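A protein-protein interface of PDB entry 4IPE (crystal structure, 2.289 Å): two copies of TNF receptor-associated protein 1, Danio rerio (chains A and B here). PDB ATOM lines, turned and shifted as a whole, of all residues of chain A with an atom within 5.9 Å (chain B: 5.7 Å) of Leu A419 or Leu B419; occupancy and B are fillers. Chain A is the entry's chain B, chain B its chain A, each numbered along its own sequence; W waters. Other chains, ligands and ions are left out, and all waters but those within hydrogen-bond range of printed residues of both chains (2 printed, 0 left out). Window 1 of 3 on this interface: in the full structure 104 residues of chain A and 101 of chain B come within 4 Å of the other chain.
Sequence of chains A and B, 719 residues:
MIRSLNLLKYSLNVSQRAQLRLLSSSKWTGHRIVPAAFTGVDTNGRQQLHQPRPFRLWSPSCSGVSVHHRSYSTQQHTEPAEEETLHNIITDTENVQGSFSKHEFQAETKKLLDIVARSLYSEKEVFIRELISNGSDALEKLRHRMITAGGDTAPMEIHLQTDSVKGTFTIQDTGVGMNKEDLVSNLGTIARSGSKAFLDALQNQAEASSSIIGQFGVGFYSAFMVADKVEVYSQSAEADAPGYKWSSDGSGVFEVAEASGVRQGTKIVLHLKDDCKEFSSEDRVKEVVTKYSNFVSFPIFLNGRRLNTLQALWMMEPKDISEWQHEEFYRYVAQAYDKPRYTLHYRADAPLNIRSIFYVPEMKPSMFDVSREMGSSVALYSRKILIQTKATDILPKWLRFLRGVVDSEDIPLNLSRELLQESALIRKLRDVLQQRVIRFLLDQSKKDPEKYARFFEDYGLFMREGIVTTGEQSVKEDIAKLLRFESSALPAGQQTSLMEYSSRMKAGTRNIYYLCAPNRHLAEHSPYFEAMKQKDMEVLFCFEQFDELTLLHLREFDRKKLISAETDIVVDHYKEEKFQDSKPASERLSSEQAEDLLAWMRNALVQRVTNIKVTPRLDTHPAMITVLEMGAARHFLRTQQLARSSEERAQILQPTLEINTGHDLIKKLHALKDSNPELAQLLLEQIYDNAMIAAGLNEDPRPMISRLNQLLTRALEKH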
ATOM      1  N   SER A 122     -16.438 -23.638  24.596  1.00  0.00           N
ATOM      2  CA  SER A 122     -15.871 -24.968  24.643  1.00  0.00           C
ATOM      3  C   SER A 122     -16.444 -25.829  25.781  1.00  0.00           C
ATOM      4  O   SER A 122     -16.335 -27.054  25.751  1.00  0.00           O
ATOM      5  CB  SER A 122     -14.350 -24.879  24.699  1.00  0.00           C
ATOM      6  OG  SER A 122     -13.898 -24.612  26.001  1.00  0.00           O
ATOM      7  N   ILE A 387     -11.658 -15.727  34.083  1.00  0.00           N
ATOM      8  CA  ILE A 387     -11.183 -15.967  32.717  1.00  0.00           C
ATOM      9  C   ILE A 387      -9.961 -16.906  32.713  1.00  0.00           C
ATOM     10  O   ILE A 387      -8.991 -16.669  33.427  1.00  0.00           O
ATOM     11  CB  ILE A 387     -10.692 -14.665  32.089  1.00  0.00           C
ATOM     12  CG1 ILE A 387     -11.666 -13.526  32.389  1.00  0.00           C
ATOM     13  CG2 ILE A 387     -10.442 -14.847  30.583  1.00  0.00           C
ATOM     14  CD1 ILE A 387     -13.019 -13.680  31.729  1.00  0.00           C
ATOM     15  N   GLN A 388      -9.975 -17.941  31.881  1.00  0.00           N
ATOM     16  CA  GLN A 388      -8.780 -18.787  31.728  1.00  0.00           C
ATOM     17  C   GLN A 388      -8.017 -18.577  30.398  1.00  0.00           C
ATOM     18  O   GLN A 388      -6.808 -18.852  30.280  1.00  0.00           O
ATOM     19  CB  GLN A 388      -9.174 -20.246  31.893  1.00  0.00           C
ATOM     20  CG  GLN A 388      -9.629 -20.590  33.311  1.00  0.00           C
ATOM     21  CD  GLN A 388     -10.079 -22.023  33.417  1.00  0.00           C
ATOM     22  OE1 GLN A 388     -10.489 -22.623  32.428  1.00  0.00           O
ATOM     23  NE2 GLN A 388      -9.988 -22.589  34.611  1.00  0.00           N
ATOM     24  N   PRO A 412      -7.578  -8.167  26.298  1.00  0.00           N
ATOM     25  CA  PRO A 412      -8.878  -8.300  25.636  1.00  0.00           C
ATOM     26  C   PRO A 412      -9.382  -9.736  25.718  1.00  0.00           C
ATOM     27  O   PRO A 412      -8.583 -10.685  25.722  1.00  0.00           O
ATOM     28  CB  PRO A 412      -8.570  -7.921  24.170  1.00  0.00           C
ATOM     29  CG  PRO A 412      -7.161  -7.335  24.184  1.00  0.00           C
ATOM     30  CD  PRO A 412      -6.484  -8.035  25.321  1.00  0.00           C
ATOM     31  N   LEU A 413     -10.700  -9.879  25.795  1.00  0.00           N
ATOM     32  CA  LEU A 413     -11.328 -11.187  25.853  1.00  0.00           C
ATOM     33  C   LEU A 413     -11.833 -11.582  24.494  1.00  0.00           C
ATOM     34  O   LEU A 413     -12.361 -10.750  23.753  1.00  0.00           O
ATOM     35  CB  LEU A 413     -12.518 -11.142  26.791  1.00  0.00           C
ATOM     36  CG  LEU A 413     -12.250 -10.732  28.221  1.00  0.00           C
ATOM     37  CD1 LEU A 413     -13.577 -10.674  28.911  1.00  0.00           C
ATOM     38  CD2 LEU A 413     -11.312 -11.720  28.908  1.00  0.00           C
ATOM     39  N   ASN A 414     -11.673 -12.863  24.178  1.00  0.00           N
ATOM     40  CA  ASN A 414     -12.261 -13.446  22.990  1.00  0.00           C
ATOM     41  C   ASN A 414     -13.769 -13.620  23.197  1.00  0.00           C
ATOM     42  O   ASN A 414     -14.256 -13.478  24.304  1.00  0.00           O
ATOM     43  CB  ASN A 414     -11.605 -14.796  22.677  1.00  0.00           C
ATOM     44  CG  ASN A 414     -11.831 -15.835  23.778  1.00  0.00           C
ATOM     45  OD1 ASN A 414     -12.264 -15.513  24.878  1.00  0.00           O
ATOM     46  ND2 ASN A 414     -11.539 -17.089  23.469  1.00  0.00           N
ATOM     47  N   SER A 416     -15.647 -16.073  23.377  1.00  0.00           N
ATOM     48  CA  SER A 416     -16.104 -17.209  24.145  1.00  0.00           C
ATOM     49  C   SER A 416     -15.834 -16.912  25.587  1.00  0.00           C
ATOM     50  O   SER A 416     -16.379 -17.575  26.470  1.00  0.00           O
ATOM     51  CB  SER A 416     -15.353 -18.468  23.721  1.00  0.00           C
ATOM     52  OG  SER A 416     -13.958 -18.249  23.834  1.00  0.00           O
ATOM     53  N   ARG A 417     -14.984 -15.909  25.808  1.00  0.00           N
ATOM     54  CA  ARG A 417     -14.600 -15.405  27.140  1.00  0.00           C
ATOM     55  C   ARG A 417     -13.705 -16.353  27.914  1.00  0.00           C
ATOM     56  O   ARG A 417     -13.786 -16.417  29.142  1.00  0.00           O
ATOM     57  CB  ARG A 417     -15.813 -15.016  28.013  1.00  0.00           C
ATOM     58  CG  ARG A 417     -16.648 -13.895  27.437  1.00  0.00           C
ATOM     59  CD  ARG A 417     -17.970 -13.716  28.154  1.00  0.00           C
ATOM     60  NE  ARG A 417     -18.572 -12.437  27.777  1.00  0.00           N
ATOM     61  CZ  ARG A 417     -18.201 -11.265  28.301  1.00  0.00           C
ATOM     62  NH1 ARG A 417     -17.238 -11.206  29.230  1.00  0.00           N
ATOM     63  NH2 ARG A 417     -18.792 -10.145  27.897  1.00  0.00           N
ATOM     64  N   GLU A 418     -12.844 -17.070  27.209  1.00  0.00           N
ATOM     65  CA  GLU A 418     -11.969 -18.026  27.873  1.00  0.00           C
ATOM     66  C   GLU A 418     -10.522 -17.960  27.377  1.00  0.00           C
ATOM     67  O   GLU A 418      -9.676 -18.738  27.811  1.00  0.00           O
ATOM     68  CB  GLU A 418     -12.530 -19.460  27.726  1.00  0.00           C
ATOM     69  CG  GLU A 418     -12.606 -19.954  26.306  1.00  0.00           C
ATOM     70  CD  GLU A 418     -13.281 -21.331  26.195  1.00  0.00           C
ATOM     71  OE1 GLU A 418     -13.374 -22.034  27.227  1.00  0.00           O
ATOM     72  OE2 GLU A 418     -13.705 -21.716  25.075  1.00  0.00           O
ATOM     73  N   LEU A 419     -10.246 -17.041  26.460  1.00  0.00           N
ATOM     74  CA  LEU A 419      -8.890 -16.863  25.940  1.00  0.00           C
ATOM     75  C   LEU A 419      -8.494 -15.384  26.010  1.00  0.00           C
ATOM     76  O   LEU A 419      -9.353 -14.498  25.921  1.00  0.00           O
ATOM     77  CB  LEU A 419      -8.795 -17.379  24.494  1.00  0.00           C
ATOM     78  CG  LEU A 419      -8.864 -18.874  24.135  1.00  0.00           C
ATOM     79  CD1 LEU A 419      -9.398 -19.049  22.724  1.00  0.00           C
ATOM     80  CD2 LEU A 419      -7.518 -19.573  24.251  1.00  0.00           C
ATOM     81  N   LEU A 420      -7.199 -15.129  26.200  1.00  0.00           N
ATOM     82  CA  LEU A 420      -6.626 -13.772  26.168  1.00  0.00           C
ATOM     83  C   LEU A 420      -6.144 -13.452  24.750  1.00  0.00           C
ATOM     84  O   LEU A 420      -5.828 -14.369  23.990  1.00  0.00           O
ATOM     85  CB  LEU A 420      -5.442 -13.702  27.119  1.00  0.00           C
ATOM     86  CG  LEU A 420      -5.861 -13.895  28.574  1.00  0.00           C
ATOM     87  CD1 LEU A 420      -4.639 -13.969  29.495  1.00  0.00           C
ATOM     88  CD2 LEU A 420      -6.829 -12.798  28.998  1.00  0.00           C
ATOM     89  N   GLN A 421      -6.045 -12.168  24.402  1.00  0.00           N
ATOM     90  CA  GLN A 421      -5.933 -11.809  22.984  1.00  0.00           C
ATOM     91  C   GLN A 421      -4.737 -11.008  22.469  1.00  0.00           C
ATOM     92  O   GLN A 421      -4.824 -10.439  21.381  1.00  0.00           O
ATOM     93  CB  GLN A 421      -7.196 -11.090  22.534  1.00  0.00           C
ATOM     94  CG  GLN A 421      -8.260 -12.003  22.021  1.00  0.00           C
ATOM     95  CD  GLN A 421      -9.384 -11.235  21.398  1.00  0.00           C
ATOM     96  OE1 GLN A 421      -9.599 -10.065  21.702  1.00  0.00           O
ATOM     97  NE2 GLN A 421     -10.108 -11.885  20.511  1.00  0.00           N
ATOM     98  N   LEU B 120     -12.315 -13.082  18.260  1.00  0.00           N
ATOM     99  CA  LEU B 120     -12.500 -14.480  17.955  1.00  0.00           C
ATOM    100  C   LEU B 120     -11.226 -15.289  18.214  1.00  0.00           C
ATOM    101  O   LEU B 120     -11.275 -16.344  18.845  1.00  0.00           O
ATOM    102  CB  LEU B 120     -12.951 -14.600  16.508  1.00  0.00           C
ATOM    103  CG  LEU B 120     -13.322 -15.975  16.012  1.00  0.00           C
ATOM    104  CD1 LEU B 120     -14.298 -16.589  17.001  1.00  0.00           C
ATOM    105  CD2 LEU B 120     -13.909 -15.863  14.587  1.00  0.00           C
ATOM    106  N   SER B 122      -7.099 -15.806  19.491  1.00  0.00           N
ATOM    107  CA  SER B 122      -6.138 -15.339  20.463  1.00  0.00           C
ATOM    108  C   SER B 122      -4.983 -14.543  19.838  1.00  0.00           C
ATOM    109  O   SER B 122      -4.322 -13.790  20.554  1.00  0.00           O
ATOM    110  CB  SER B 122      -5.582 -16.512  21.251  1.00  0.00           C
ATOM    111  OG  SER B 122      -4.709 -17.266  20.435  1.00  0.00           O
ATOM    112  N   ILE B 387      -4.158 -27.320  15.287  1.00  0.00           N
ATOM    113  CA  ILE B 387      -5.191 -26.816  16.209  1.00  0.00           C
ATOM    114  C   ILE B 387      -4.555 -26.283  17.505  1.00  0.00           C
ATOM    115  O   ILE B 387      -4.819 -25.151  17.910  1.00  0.00           O
ATOM    116  CB  ILE B 387      -6.248 -27.900  16.544  1.00  0.00           C
ATOM    117  CG1 ILE B 387      -6.763 -28.563  15.261  1.00  0.00           C
ATOM    118  CG2 ILE B 387      -7.417 -27.280  17.297  1.00  0.00           C
ATOM    119  CD1 ILE B 387      -7.519 -27.579  14.347  1.00  0.00           C
ATOM    120  N   GLN B 388      -3.703 -27.096  18.133  1.00  0.00           N
ATOM    121  CA  GLN B 388      -3.064 -26.751  19.403  1.00  0.00           C
ATOM    122  C   GLN B 388      -1.644 -27.317  19.453  1.00  0.00           C
ATOM    123  O   GLN B 388      -1.462 -28.534  19.289  1.00  0.00           O
ATOM    124  CB  GLN B 388      -3.831 -27.386  20.573  1.00  0.00           C
ATOM    125  CG  GLN B 388      -5.194 -26.812  20.872  1.00  0.00           C
ATOM    126  CD  GLN B 388      -5.886 -27.552  22.020  1.00  0.00           C
ATOM    127  OE1 GLN B 388      -5.663 -28.746  22.241  1.00  0.00           O
ATOM    128  NE2 GLN B 388      -6.725 -26.839  22.754  1.00  0.00           N
ATOM    129  N   PRO B 412     -14.785 -32.304  17.088  1.00  0.00           N
ATOM    130  CA  PRO B 412     -15.589 -31.072  17.118  1.00  0.00           C
ATOM    131  C   PRO B 412     -14.754 -29.825  17.486  1.00  0.00           C
ATOM    132  O   PRO B 412     -14.302 -29.719  18.625  1.00  0.00           O
ATOM    133  CB  PRO B 412     -16.638 -31.351  18.215  1.00  0.00           C
ATOM    134  CG  PRO B 412     -16.410 -32.797  18.656  1.00  0.00           C
ATOM    135  CD  PRO B 412     -15.044 -33.185  18.244  1.00  0.00           C
ATOM    136  N   LEU B 413     -14.580 -28.898  16.545  1.00  0.00           N
ATOM    137  CA  LEU B 413     -13.710 -27.739  16.765  1.00  0.00           C
ATOM    138  C   LEU B 413     -14.488 -26.555  17.287  1.00  0.00           C
ATOM    139  O   LEU B 413     -15.660 -26.329  16.931  1.00  0.00           O
ATOM    140  CB  LEU B 413     -13.004 -27.324  15.475  1.00  0.00           C
ATOM    141  CG  LEU B 413     -12.104 -28.345  14.795  1.00  0.00           C
ATOM    142  CD1 LEU B 413     -11.688 -27.778  13.447  1.00  0.00           C
ATOM    143  CD2 LEU B 413     -10.882 -28.735  15.639  1.00  0.00           C
ATOM    144  N   ASN B 414     -13.847 -25.789  18.154  1.00  0.00           N
ATOM    145  CA  ASN B 414     -14.414 -24.528  18.587  1.00  0.00           C
ATOM    146  C   ASN B 414     -14.276 -23.592  17.388  1.00  0.00           C
ATOM    147  O   ASN B 414     -13.386 -23.804  16.547  1.00  0.00           O
ATOM    148  CB  ASN B 414     -13.588 -24.018  19.772  1.00  0.00           C
ATOM    149  CG  ASN B 414     -14.099 -22.713  20.304  1.00  0.00           C
ATOM    150  OD1 ASN B 414     -13.688 -21.647  19.845  1.00  0.00           O
ATOM    151  ND2 ASN B 414     -15.019 -22.777  21.278  1.00  0.00           N
ATOM    152  N   SER B 416     -12.942 -20.798  17.092  1.00  0.00           N
ATOM    153  CA  SER B 416     -11.645 -20.142  17.007  1.00  0.00           C
ATOM    154  C   SER B 416     -10.606 -21.060  16.377  1.00  0.00           C
ATOM    155  O   SER B 416      -9.515 -20.618  16.091  1.00  0.00           O
ATOM    156  CB  SER B 416     -11.150 -19.772  18.401  1.00  0.00           C
ATOM    157  OG  SER B 416     -10.811 -20.960  19.115  1.00  0.00           O
ATOM    158  N   ARG B 417     -10.946 -22.337  16.219  1.00  0.00           N
ATOM    159  CA  ARG B 417     -10.018 -23.334  15.692  1.00  0.00           C
ATOM    160  C   ARG B 417      -8.719 -23.457  16.488  1.00  0.00           C
ATOM    161  O   ARG B 417      -7.677 -23.872  15.956  1.00  0.00           O
ATOM    162  CB  ARG B 417      -9.697 -23.068  14.222  1.00  0.00           C
ATOM    163  CG  ARG B 417     -10.884 -23.249  13.325  1.00  0.00           C
ATOM    164  CD  ARG B 417     -10.574 -22.833  11.893  1.00  0.00           C
ATOM    165  NE  ARG B 417     -11.696 -23.209  11.054  1.00  0.00           N
ATOM    166  CZ  ARG B 417     -11.882 -24.441  10.601  1.00  0.00           C
ATOM    167  NH1 ARG B 417     -11.002 -25.419  10.879  1.00  0.00           N
ATOM    168  NH2 ARG B 417     -12.937 -24.707   9.843  1.00  0.00           N
ATOM    169  N   GLU B 418      -8.771 -23.100  17.761  1.00  0.00           N
ATOM    170  CA  GLU B 418      -7.619 -23.344  18.617  1.00  0.00           C
ATOM    171  C   GLU B 418      -8.037 -24.063  19.912  1.00  0.00           C
ATOM    172  O   GLU B 418      -7.246 -24.164  20.839  1.00  0.00           O
ATOM    173  CB  GLU B 418      -6.864 -22.036  18.894  1.00  0.00           C
ATOM    174  CG  GLU B 418      -7.642 -21.030  19.704  1.00  0.00           C
ATOM    175  CD  GLU B 418      -6.905 -19.697  19.872  1.00  0.00           C
ATOM    176  OE1 GLU B 418      -7.331 -18.689  19.254  1.00  0.00           O
ATOM    177  OE2 GLU B 418      -5.917 -19.657  20.648  1.00  0.00           O
ATOM    178  N   LEU B 419      -9.278 -24.559  19.945  1.00  0.00           N
ATOM    179  CA  LEU B 419      -9.806 -25.334  21.072  1.00  0.00           C
ATOM    180  C   LEU B 419     -10.744 -26.393  20.522  1.00  0.00           C
ATOM    181  O   LEU B 419     -11.230 -26.267  19.394  1.00  0.00           O
ATOM    182  CB  LEU B 419     -10.630 -24.452  22.023  1.00  0.00           C
ATOM    183  CG  LEU B 419      -9.930 -23.324  22.762  1.00  0.00           C
ATOM    184  CD1 LEU B 419     -10.942 -22.410  23.480  1.00  0.00           C
ATOM    185  CD2 LEU B 419      -8.924 -23.926  23.739  1.00  0.00           C
ATOM    186  N   LEU B 420     -11.019 -27.399  21.354  1.00  0.00           N
ATOM    187  CA  LEU B 420     -12.014 -28.433  21.077  1.00  0.00           C
ATOM    188  C   LEU B 420     -13.233 -28.197  21.917  1.00  0.00           C
ATOM    189  O   LEU B 420     -13.139 -27.711  23.034  1.00  0.00           O
ATOM    190  CB  LEU B 420     -11.464 -29.786  21.463  1.00  0.00           C
ATOM    191  CG  LEU B 420     -10.276 -30.220  20.627  1.00  0.00           C
ATOM    192  CD1 LEU B 420      -9.887 -31.595  21.117  1.00  0.00           C
ATOM    193  CD2 LEU B 420     -10.637 -30.202  19.136  1.00  0.00           C
ATOM    194  N   GLN B 421     -14.385 -28.537  21.364  1.00  0.00           N
ATOM    195  CA  GLN B 421     -15.631 -28.451  22.107  1.00  0.00           C
ATOM    196  C   GLN B 421     -15.671 -29.592  23.107  1.00  0.00           C
ATOM    197  O   GLN B 421     -15.006 -30.618  22.907  1.00  0.00           O
ATOM    198  CB  GLN B 421     -16.823 -28.531  21.146  1.00  0.00           C
ATOM    199  CG  GLN B 421     -16.934 -27.326  20.215  1.00  0.00           C
ATOM    200  CD  GLN B 421     -16.995 -26.036  21.013  1.00  0.00           C
ATOM    201  OE1 GLN B 421     -15.968 -25.445  21.343  1.00  0.00           O
ATOM    202  NE2 GLN B 421     -18.207 -25.612  21.354  1.00  0.00           N
HETATM  203  O   HOH W   1     -14.663 -19.393  20.795  1.00  0.00           O
HETATM  204  O   HOH W   2     -13.397 -17.028  20.755  1.00  0.00           O
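OG of Ser B122 sits at hydrogen-bond distance from OE2 of Glu B418. The backbone carbonyl oxygen of Glu B418 sits at hydrogen-bond distance from the side-chain amide nitrogen of Gln B388. The backbone carbonyl oxygen (O) of Pro B412 lies within hydrogen-bond range of the backbone NH (N) of Gln B421. O of Leu B419 is in hydrogen-bond range of N of Asn B414 (2.9 Å). OG of Ser A122 lies within hydrogen-bond range of OE1 of Glu A418 (2.9 Å). The side-chain amide oxygen (OD1) of Asn A414 is in hydrogen-bond range of the backbone NH (N) of Glu A418, 2.9 Å away.
Water W1 bridges OD1 of Asn B414 and OG of Ser A416. Water W2 lies within hydrogen-bond range of O of Leu B120 (2.9 Å), ND2 of Asn A414 (3.3 Å) and OG of Ser A416 (3.4 Å).
Ser A122 touches Leu B420, and with the chains exchanged Leu A420 touches Ser B122. Ser A122 touches Gln B421, and with the chains exchanged Gln A421 touches Ser B122. Glu A418 touches Leu B419, and with the chains exchanged Leu A419 touches Glu B418. Leu B419 touches its own counterpart, Leu A419. Positions printed for both chains: 122, 387, 388, 412, 413, 414, 416, 417, 418, 419, 420 and 421.
Leu A419 touches just these residues of chain B: Glu B418 (3.8 Å) and Leu B419 (3.8 Å). Leu B419 touches just these residues of chain A: Glu A418 and Leu A419. Printed residues of chain B within 4 Å of Leu A420: Ser B122 (3.5 Å). Of the printed residues of chain A, Leu B420 touches Ser A122 (3.5 Å). Printed residues of chain A within 4 Å of Asn B414: Ser A122. Printed residues of chain A within 4 Å of Ser B122: Leu A420 and Gln A421. Gln B388 touches none of the printed residues of chain A. Leu A413 touches none of the printed residues of chain B. The nearest residue of chain B that does not touch Leu A419 is Ser B416 (4.3 Å). The nearest residue of chain A that does not touch Leu B419 is Ser A122 (4.4 Å).
Hydrophobic or aromatic side chains of chain A within 4 Å of the printed part of chain B: Leu A419. Hydrophobic or aromatic side chains of chain B within 4 Å of the printed part of chain A: Leu B419. Among the printed residues, 9 pairs touch across the chains. Among the printed residues, no Asp or Glu carboxylate lies within 4 Å of a Lys or Arg side-chain nitrogen of the other chain.
Among the printed residues, pairs that only touch across the chains: Ser A122 with Asn B414, Ser A122 with Leu B420, Ser A122 with Gln B421, Glu A418 with Leu B419, Leu A419 with Glu B418, Leu A419 with Leu B419 and Leu A420 with Ser B122.
N of Leu B120 lies close to NE2 of Gln A421, at 3.4 Å. The backbone carbonyl oxygen (O) of Gln A421 sits close to the backbone carbonyl oxygen (O) of Ser B122, 3.5 Å away.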
